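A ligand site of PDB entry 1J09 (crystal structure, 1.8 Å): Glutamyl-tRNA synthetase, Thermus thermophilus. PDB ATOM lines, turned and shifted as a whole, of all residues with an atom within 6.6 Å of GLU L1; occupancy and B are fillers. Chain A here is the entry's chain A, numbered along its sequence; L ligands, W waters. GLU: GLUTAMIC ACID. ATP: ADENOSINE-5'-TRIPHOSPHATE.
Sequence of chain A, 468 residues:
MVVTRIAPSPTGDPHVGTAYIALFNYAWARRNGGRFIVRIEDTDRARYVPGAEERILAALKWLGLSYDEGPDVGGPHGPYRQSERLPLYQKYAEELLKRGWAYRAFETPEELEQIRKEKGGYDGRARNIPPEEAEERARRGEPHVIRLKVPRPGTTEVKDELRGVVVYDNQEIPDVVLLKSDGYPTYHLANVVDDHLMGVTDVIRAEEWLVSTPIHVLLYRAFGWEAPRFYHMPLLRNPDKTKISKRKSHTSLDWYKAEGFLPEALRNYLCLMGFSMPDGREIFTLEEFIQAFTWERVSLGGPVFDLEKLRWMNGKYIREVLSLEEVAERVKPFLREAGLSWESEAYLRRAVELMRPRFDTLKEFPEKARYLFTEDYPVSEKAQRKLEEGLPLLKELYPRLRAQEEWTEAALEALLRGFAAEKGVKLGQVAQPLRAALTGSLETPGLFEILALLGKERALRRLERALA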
ATOM      1  N   ARG A   5     -14.600 -11.590  -0.439  1.00  0.00           N
ATOM      2  CA  ARG A   5     -14.662 -10.453   0.469  1.00  0.00           C
ATOM      3  C   ARG A   5     -13.915 -10.695   1.778  1.00  0.00           C
ATOM      4  O   ARG A   5     -13.456 -11.796   2.054  1.00  0.00           O
ATOM      5  CB  ARG A   5     -16.127 -10.132   0.796  1.00  0.00           C
ATOM      6  CG  ARG A   5     -17.005 -11.320   1.272  1.00  0.00           C
ATOM      7  CD  ARG A   5     -16.515 -11.984   2.561  1.00  0.00           C
ATOM      8  NE  ARG A   5     -17.576 -12.667   3.299  1.00  0.00           N
ATOM      9  CZ  ARG A   5     -17.391 -13.332   4.436  1.00  0.00           C
ATOM     10  NH1 ARG A   5     -16.177 -13.423   4.970  1.00  0.00           N
ATOM     11  NH2 ARG A   5     -18.424 -13.897   5.060  1.00  0.00           N
ATOM     12  N   ILE A   6     -13.754  -9.621   2.547  1.00  0.00           N
ATOM     13  CA  ILE A   6     -13.241  -9.737   3.899  1.00  0.00           C
ATOM     14  C   ILE A   6     -14.336  -8.986   4.628  1.00  0.00           C
ATOM     15  O   ILE A   6     -14.920  -8.036   4.088  1.00  0.00           O
ATOM     16  CB  ILE A   6     -11.866  -9.075   4.141  1.00  0.00           C
ATOM     17  CG1 ILE A   6     -11.820  -7.661   3.586  1.00  0.00           C
ATOM     18  CG2 ILE A   6     -10.779  -9.993   3.617  1.00  0.00           C
ATOM     19  CD1 ILE A   6     -10.566  -6.916   4.017  1.00  0.00           C
ATOM     20  N   ALA A   7     -14.655  -9.428   5.831  1.00  0.00           N
ATOM     21  CA  ALA A   7     -15.716  -8.787   6.607  1.00  0.00           C
ATOM     22  C   ALA A   7     -15.199  -8.536   8.010  1.00  0.00           C
ATOM     23  O   ALA A   7     -15.720  -9.087   8.990  1.00  0.00           O
ATOM     24  CB  ALA A   7     -16.945  -9.694   6.656  1.00  0.00           C
ATOM     25  N   PRO A   8     -14.167  -7.700   8.131  1.00  0.00           N
ATOM     26  CA  PRO A   8     -13.595  -7.403   9.442  1.00  0.00           C
ATOM     27  C   PRO A   8     -14.561  -6.679  10.364  1.00  0.00           C
ATOM     28  O   PRO A   8     -15.366  -5.842   9.934  1.00  0.00           O
ATOM     29  CB  PRO A   8     -12.377  -6.556   9.109  1.00  0.00           C
ATOM     30  CG  PRO A   8     -12.833  -5.808   7.882  1.00  0.00           C
ATOM     31  CD  PRO A   8     -13.514  -6.897   7.080  1.00  0.00           C
ATOM     32  N   SER A   9     -14.467  -7.020  11.639  1.00  0.00           N
ATOM     33  CA  SER A   9     -15.251  -6.394  12.685  1.00  0.00           C
ATOM     34  C   SER A   9     -14.185  -5.603  13.438  1.00  0.00           C
ATOM     35  O   SER A   9     -13.451  -6.159  14.264  1.00  0.00           O
ATOM     36  CB  SER A   9     -15.883  -7.460  13.596  1.00  0.00           C
ATOM     37  OG  SER A   9     -16.895  -8.178  12.915  1.00  0.00           O
ATOM     38  N   ILE A  21      -6.182 -13.445   5.983  1.00  0.00           N
ATOM     39  CA  ILE A  21      -7.401 -13.849   5.277  1.00  0.00           C
ATOM     40  C   ILE A  21      -7.631 -12.982   4.048  1.00  0.00           C
ATOM     41  O   ILE A  21      -8.037 -13.487   2.994  1.00  0.00           O
ATOM     42  CB  ILE A  21      -8.631 -13.759   6.206  1.00  0.00           C
ATOM     43  CG1 ILE A  21      -8.472 -14.739   7.368  1.00  0.00           C
ATOM     44  CG2 ILE A  21      -9.910 -14.032   5.428  1.00  0.00           C
ATOM     45  CD1 ILE A  21      -8.302 -16.196   6.944  1.00  0.00           C
ATOM     46  N   ARG A  39     -16.308  -5.386   3.444  1.00  0.00           N
ATOM     47  CA  ARG A  39     -17.523  -5.043   4.174  1.00  0.00           C
ATOM     48  C   ARG A  39     -17.133  -4.872   5.639  1.00  0.00           C
ATOM     49  O   ARG A  39     -16.459  -5.736   6.206  1.00  0.00           O
ATOM     50  CB  ARG A  39     -18.601  -6.126   4.048  1.00  0.00           C
ATOM     51  CG  ARG A  39     -19.841  -5.819   4.885  1.00  0.00           C
ATOM     52  CD  ARG A  39     -20.954  -6.847   4.697  1.00  0.00           C
ATOM     53  NE  ARG A  39     -20.607  -8.164   5.231  1.00  0.00           N
ATOM     54  CZ  ARG A  39     -20.529  -9.258   4.486  1.00  0.00           C
ATOM     55  NH1 ARG A  39     -20.759  -9.213   3.177  1.00  0.00           N
ATOM     56  NH2 ARG A  39     -20.249 -10.429   5.055  1.00  0.00           N
ATOM     57  N   GLU A  41     -18.088  -4.963   9.368  1.00  0.00           N
ATOM     58  CA  GLU A  41     -19.125  -5.480  10.244  1.00  0.00           C
ATOM     59  C   GLU A  41     -18.911  -4.785  11.583  1.00  0.00           C
ATOM     60  O   GLU A  41     -18.277  -5.314  12.509  1.00  0.00           O
ATOM     61  CB  GLU A  41     -19.002  -7.013  10.335  1.00  0.00           C
ATOM     62  CG  GLU A  41     -18.965  -7.671   8.946  1.00  0.00           C
ATOM     63  CD  GLU A  41     -19.499  -9.089   8.919  1.00  0.00           C
ATOM     64  OE1 GLU A  41     -19.328  -9.830   9.908  1.00  0.00           O
ATOM     65  OE2 GLU A  41     -20.078  -9.468   7.879  1.00  0.00           O
ATOM     66  N   GLN A  82     -22.082  -2.381   8.018  1.00  0.00           N
ATOM     67  CA  GLN A  82     -23.308  -2.982   8.502  1.00  0.00           C
ATOM     68  C   GLN A  82     -24.104  -2.024   9.383  1.00  0.00           C
ATOM     69  O   GLN A  82     -25.322  -2.145   9.506  1.00  0.00           O
ATOM     70  CB  GLN A  82     -22.997  -4.308   9.203  1.00  0.00           C
ATOM     71  CG  GLN A  82     -22.497  -5.350   8.205  1.00  0.00           C
ATOM     72  CD  GLN A  82     -22.432  -6.764   8.770  1.00  0.00           C
ATOM     73  OE1 GLN A  82     -22.630  -7.747   8.047  1.00  0.00           O
ATOM     74  NE2 GLN A  82     -22.140  -6.885  10.057  1.00  0.00           N
ATOM     75  N   TYR A 187     -24.169 -11.853  14.188  1.00  0.00           N
ATOM     76  CA  TYR A 187     -23.281 -12.165  13.087  1.00  0.00           C
ATOM     77  C   TYR A 187     -23.902 -13.080  12.021  1.00  0.00           C
ATOM     78  O   TYR A 187     -23.778 -12.812  10.831  1.00  0.00           O
ATOM     79  CB  TYR A 187     -22.016 -12.824  13.653  1.00  0.00           C
ATOM     80  CG  TYR A 187     -21.260 -13.677  12.661  1.00  0.00           C
ATOM     81  CD1 TYR A 187     -20.555 -13.088  11.609  1.00  0.00           C
ATOM     82  CD2 TYR A 187     -21.263 -15.065  12.771  1.00  0.00           C
ATOM     83  CE1 TYR A 187     -19.873 -13.878  10.689  1.00  0.00           C
ATOM     84  CE2 TYR A 187     -20.581 -15.865  11.861  1.00  0.00           C
ATOM     85  CZ  TYR A 187     -19.886 -15.265  10.822  1.00  0.00           C
ATOM     86  OH  TYR A 187     -19.214 -16.054   9.924  1.00  0.00           O
ATOM     87  N   ASN A 191     -24.215 -11.534   8.298  1.00  0.00           N
ATOM     88  CA  ASN A 191     -23.219 -12.095   7.397  1.00  0.00           C
ATOM     89  C   ASN A 191     -23.846 -12.758   6.164  1.00  0.00           C
ATOM     90  O   ASN A 191     -23.390 -12.547   5.044  1.00  0.00           O
ATOM     91  CB  ASN A 191     -22.345 -13.099   8.157  1.00  0.00           C
ATOM     92  CG  ASN A 191     -21.048 -13.408   7.433  1.00  0.00           C
ATOM     93  OD1 ASN A 191     -20.910 -14.466   6.813  1.00  0.00           O
ATOM     94  ND2 ASN A 191     -20.091 -12.485   7.510  1.00  0.00           N
ATOM     95  N   ASP A 195     -23.623 -11.143   2.406  1.00  0.00           N
ATOM     96  CA  ASP A 195     -22.851 -11.870   1.410  1.00  0.00           C
ATOM     97  C   ASP A 195     -23.771 -12.102   0.211  1.00  0.00           C
ATOM     98  O   ASP A 195     -23.353 -12.027  -0.943  1.00  0.00           O
ATOM     99  CB  ASP A 195     -22.359 -13.212   1.943  1.00  0.00           C
ATOM    100  CG  ASP A 195     -21.067 -13.096   2.731  1.00  0.00           C
ATOM    101  OD1 ASP A 195     -20.652 -14.100   3.324  1.00  0.00           O
ATOM    102  OD2 ASP A 195     -20.471 -11.992   2.745  1.00  0.00           O
ATOM    103  N   VAL A 203     -16.633 -17.662  -0.139  1.00  0.00           N
ATOM    104  CA  VAL A 203     -16.376 -17.217   1.225  1.00  0.00           C
ATOM    105  C   VAL A 203     -15.114 -17.896   1.759  1.00  0.00           C
ATOM    106  O   VAL A 203     -15.095 -19.101   1.974  1.00  0.00           O
ATOM    107  CB  VAL A 203     -17.559 -17.553   2.149  1.00  0.00           C
ATOM    108  CG1 VAL A 203     -17.216 -17.224   3.607  1.00  0.00           C
ATOM    109  CG2 VAL A 203     -18.783 -16.768   1.708  1.00  0.00           C
ATOM    110  N   ILE A 204     -14.069 -17.096   1.954  1.00  0.00           N
ATOM    111  CA  ILE A 204     -12.798 -17.587   2.468  1.00  0.00           C
ATOM    112  C   ILE A 204     -12.570 -16.920   3.829  1.00  0.00           C
ATOM    113  O   ILE A 204     -12.459 -15.692   3.918  1.00  0.00           O
ATOM    114  CB  ILE A 204     -11.647 -17.213   1.515  1.00  0.00           C
ATOM    115  CG1 ILE A 204     -11.918 -17.820   0.129  1.00  0.00           C
ATOM    116  CG2 ILE A 204     -10.300 -17.685   2.091  1.00  0.00           C
ATOM    117  CD1 ILE A 204     -11.063 -17.221  -0.999  1.00  0.00           C
ATOM    118  N   ARG A 205     -12.521 -17.719   4.882  1.00  0.00           N
ATOM    119  CA  ARG A 205     -12.340 -17.187   6.231  1.00  0.00           C
ATOM    120  C   ARG A 205     -11.609 -18.170   7.139  1.00  0.00           C
ATOM    121  O   ARG A 205     -11.417 -19.334   6.768  1.00  0.00           O
ATOM    122  CB  ARG A 205     -13.709 -16.833   6.826  1.00  0.00           C
ATOM    123  CG  ARG A 205     -14.684 -18.026   6.850  1.00  0.00           C
ATOM    124  CD  ARG A 205     -16.112 -17.582   7.208  1.00  0.00           C
ATOM    125  NE  ARG A 205     -17.060 -18.698   7.217  1.00  0.00           N
ATOM    126  CZ  ARG A 205     -18.375 -18.537   7.182  1.00  0.00           C
ATOM    127  NH1 ARG A 205     -18.877 -17.311   7.120  1.00  0.00           N
ATOM    128  NH2 ARG A 205     -19.196 -19.591   7.192  1.00  0.00           N
ATOM    129  N   ALA A 206     -11.213 -17.705   8.315  1.00  0.00           N
ATOM    130  CA  ALA A 206     -10.482 -18.542   9.280  1.00  0.00           C
ATOM    131  C   ALA A 206     -11.320 -19.736   9.747  1.00  0.00           C
ATOM    132  O   ALA A 206     -12.543 -19.633   9.886  1.00  0.00           O
ATOM    133  CB  ALA A 206     -10.063 -17.686  10.470  1.00  0.00           C
ATOM    134  N   GLU A 208     -11.954 -20.957  12.489  1.00  0.00           N
ATOM    135  CA  GLU A 208     -12.755 -20.808  13.697  1.00  0.00           C
ATOM    136  C   GLU A 208     -14.217 -20.531  13.360  1.00  0.00           C
ATOM    137  O   GLU A 208     -15.100 -20.643  14.218  1.00  0.00           O
ATOM    138  CB  GLU A 208     -12.191 -19.703  14.609  1.00  0.00           C
ATOM    139  CG  GLU A 208     -12.267 -18.278  14.057  1.00  0.00           C
ATOM    140  CD  GLU A 208     -11.780 -17.254  15.057  1.00  0.00           C
ATOM    141  OE1 GLU A 208     -11.552 -17.635  16.226  1.00  0.00           O
ATOM    142  OE2 GLU A 208     -11.610 -16.078  14.691  1.00  0.00           O
ATOM    143  N   TRP A 209     -14.483 -20.177  12.106  1.00  0.00           N
ATOM    144  CA  TRP A 209     -15.856 -19.904  11.673  1.00  0.00           C
ATOM    145  C   TRP A 209     -16.506 -21.142  11.061  1.00  0.00           C
ATOM    146  O   TRP A 209     -17.700 -21.145  10.784  1.00  0.00           O
ATOM    147  CB  TRP A 209     -15.868 -18.755  10.650  1.00  0.00           C
ATOM    148  CG  TRP A 209     -15.290 -17.469  11.177  1.00  0.00           C
ATOM    149  CD1 TRP A 209     -14.040 -16.971  10.930  1.00  0.00           C
ATOM    150  CD2 TRP A 209     -15.914 -16.569  12.092  1.00  0.00           C
ATOM    151  NE1 TRP A 209     -13.855 -15.806  11.638  1.00  0.00           N
ATOM    152  CE2 TRP A 209     -14.991 -15.536  12.356  1.00  0.00           C
ATOM    153  CE3 TRP A 209     -17.176 -16.523  12.705  1.00  0.00           C
ATOM    154  CZ2 TRP A 209     -15.278 -14.470  13.224  1.00  0.00           C
ATOM    155  CZ3 TRP A 209     -17.457 -15.463  13.566  1.00  0.00           C
ATOM    156  CH2 TRP A 209     -16.518 -14.447  13.811  1.00  0.00           C
ATOM    157  N   HIS A 216     -25.383 -20.953   8.704  1.00  0.00           N
ATOM    158  CA  HIS A 216     -25.459 -20.133   7.501  1.00  0.00           C
ATOM    159  C   HIS A 216     -26.156 -20.875   6.376  1.00  0.00           C
ATOM    160  O   HIS A 216     -26.945 -20.290   5.636  1.00  0.00           O
ATOM    161  CB  HIS A 216     -24.049 -19.693   7.107  1.00  0.00           C
ATOM    162  CG  HIS A 216     -23.332 -18.964   8.197  1.00  0.00           C
ATOM    163  ND1 HIS A 216     -21.977 -18.705   8.171  1.00  0.00           N
ATOM    164  CD2 HIS A 216     -23.784 -18.464   9.375  1.00  0.00           C
ATOM    165  CE1 HIS A 216     -21.625 -18.072   9.271  1.00  0.00           C
ATOM    166  NE2 HIS A 216     -22.705 -17.906  10.018  1.00  0.00           N
HETATM  167  N   GLU L   1     -16.858 -10.207  11.044  1.00  0.00           N
HETATM  168  CA  GLU L   1     -16.425 -11.600  11.105  1.00  0.00           C
HETATM  169  C   GLU L   1     -14.966 -11.662  11.592  1.00  0.00           C
HETATM  170  O   GLU L   1     -14.654 -10.893  12.521  1.00  0.00           O
HETATM  171  CB  GLU L   1     -16.574 -12.241   9.723  1.00  0.00           C
HETATM  172  CG  GLU L   1     -16.382 -13.749   9.691  1.00  0.00           C
HETATM  173  CD  GLU L   1     -16.652 -14.329   8.312  1.00  0.00           C
HETATM  174  OE1 GLU L   1     -17.798 -14.754   8.045  1.00  0.00           O
HETATM  175  OE2 GLU L   1     -15.713 -14.345   7.489  1.00  0.00           O
HETATM  176  OXT GLU L   1     -14.107 -12.253  10.889  1.00  0.00           O
HETATM  177  PG  ATP L   2      -9.592 -13.019  20.948  1.00  0.00           P
HETATM  178  O1G ATP L   2     -10.696 -13.764  20.216  1.00  0.00           O
HETATM  179  O2G ATP L   2      -8.614 -14.013  21.534  1.00  0.00           O
HETATM  180  O3G ATP L   2     -10.202 -12.179  22.053  1.00  0.00           O
HETATM  181  PB  ATP L   2      -8.428 -12.487  18.390  1.00  0.00           P
HETATM  182  O1B ATP L   2      -9.236 -13.656  17.995  1.00  0.00           O
HETATM  183  O2B ATP L   2      -6.942 -12.545  18.330  1.00  0.00           O
HETATM  184  O3B ATP L   2      -8.809 -12.034  19.918  1.00  0.00           O
HETATM  185  PA  ATP L   2     -10.412 -10.953  17.038  1.00  0.00           P
HETATM  186  O1A ATP L   2     -11.269 -11.902  17.788  1.00  0.00           O
HETATM  187  O2A ATP L   2     -10.646  -9.485  17.166  1.00  0.00           O
HETATM  188  O3A ATP L   2      -8.864 -11.204  17.485  1.00  0.00           O
HETATM  189  O5' ATP L   2     -10.438 -11.354  15.493  1.00  0.00           O
HETATM  190  C5' ATP L   2     -10.042 -10.433  14.489  1.00  0.00           C
HETATM  191  C4' ATP L   2     -10.009 -11.106  13.126  1.00  0.00           C
HETATM  192  O4' ATP L   2      -8.821 -11.939  13.033  1.00  0.00           O
HETATM  193  C3' ATP L   2     -11.182 -12.022  12.805  1.00  0.00           C
HETATM  194  O3' ATP L   2     -11.462 -11.971  11.404  1.00  0.00           O
HETATM  195  C2' ATP L   2     -10.656 -13.390  13.217  1.00  0.00           C
HETATM  196  O2' ATP L   2     -11.287 -14.487  12.574  1.00  0.00           O
HETATM  197  C1' ATP L   2      -9.189 -13.284  12.809  1.00  0.00           C
HETATM  198  N9  ATP L   2      -8.295 -14.128  13.599  1.00  0.00           N
HETATM  199  C8  ATP L   2      -8.141 -14.142  14.959  1.00  0.00           C
HETATM  200  N7  ATP L   2      -7.232 -14.989  15.389  1.00  0.00           N
HETATM  201  C5  ATP L   2      -6.761 -15.573  14.224  1.00  0.00           C
HETATM  202  C6  ATP L   2      -5.778 -16.562  13.993  1.00  0.00           C
HETATM  203  N6  ATP L   2      -5.076 -17.150  14.963  1.00  0.00           N
HETATM  204  N1  ATP L   2      -5.547 -16.931  12.708  1.00  0.00           N
HETATM  205  C2  ATP L   2      -6.266 -16.344  11.740  1.00  0.00           C
HETATM  206  N3  ATP L   2      -7.216 -15.412  11.828  1.00  0.00           N
HETATM  207  C4  ATP L   2      -7.413 -15.066  13.115  1.00  0.00           C
HETATM  208  O   HOH W   1     -12.681  -9.061  12.562  1.00  0.00           O
HETATM  209  O   HOH W   2     -13.720 -11.827  15.041  1.00  0.00           O
HETATM  210  O   HOH W   3     -13.527 -13.347   8.480  1.00  0.00           O
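The backbone carbonyl oxygen (O) of Ala 7 sits at hydrogen-bond distance from a nitrogen (N) of GLU L1, 2.6 Å away. OE1 of GLU L1 is in hydrogen-bond range of OH of Tyr 187, 2.7 Å away. The guanidinium group (NH1) of Arg 5 is in salt-bridge range of an oxygen (OE2) of GLU L1 (2.7 Å). The side-chain carboxylate (OE1) of Glu 41 lies within salt-bridge range of a nitrogen (N) of GLU L1 (2.7 Å). OG of Ser 9 sits at hydrogen-bond distance from N of GLU L1. NH1 of Arg 205 is in salt-bridge range of OE1 of GLU L1 (2.9 Å). OE1 of GLU L1 is in hydrogen-bond range of ND2 of Asn 191, 3.3 Å away. The indole nitrogen (NE1) of Trp 209 is in hydrogen-bond range of an oxygen (O2') of ATP L2. OE2 of Glu 208 sits at hydrogen-bond distance from O2' of ATP L2 (2.7 Å).
OXT of GLU L1 lies within hydrogen-bond range of O3' of ATP L2, 2.7 Å away.
The side-chain hydroxyl of Tyr 187 is in hydrogen-bond range of the guanidinium group of Arg 205, at 3.1 Å. NH2 of Arg 5 sits at hydrogen-bond distance from OD1 of Asn 191 (3.1 Å). The guanidinium group of Arg 5 is in salt-bridge range of the side-chain carboxylate of Asp 195. ND2 of Asn 191 sits at hydrogen-bond distance from OE2 of Glu 41, 3.0 Å away. N of Glu 41 sits at hydrogen-bond distance from O of Pro 8 (2.9 Å). The side-chain carboxylate (OE2) of Glu 41 lies close to the side-chain amide oxygen (OE1) of Gln 82 (3.1 Å). The guanidinium group (NH2) of Arg 205 is in hydrogen-bond range of a ring nitrogen (ND1) of His 216, at 3.1 Å. NH2 of Arg 39 lies close to ND2 of Asn 191, 3.2 Å away.
Trp 209 touches GLU L1. Hydrophobic or aromatic side chains that line GLU L1: Tyr 187 and Trp 209. Eight residues have an atom within 4 Å of GLU L1: Arg 5, Ala 7, Ser 9, Glu 41, Tyr 187, Asn 191, Arg 205 and Trp 209.
Water W1 lies within hydrogen-bond range of an oxygen (O) of GLU L1, the backbone NH of Ser 9 and an oxygen (O3') of ATP L2. Water W2 lies within hydrogen-bond range of O of GLU L1 and O5' of ATP L2.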
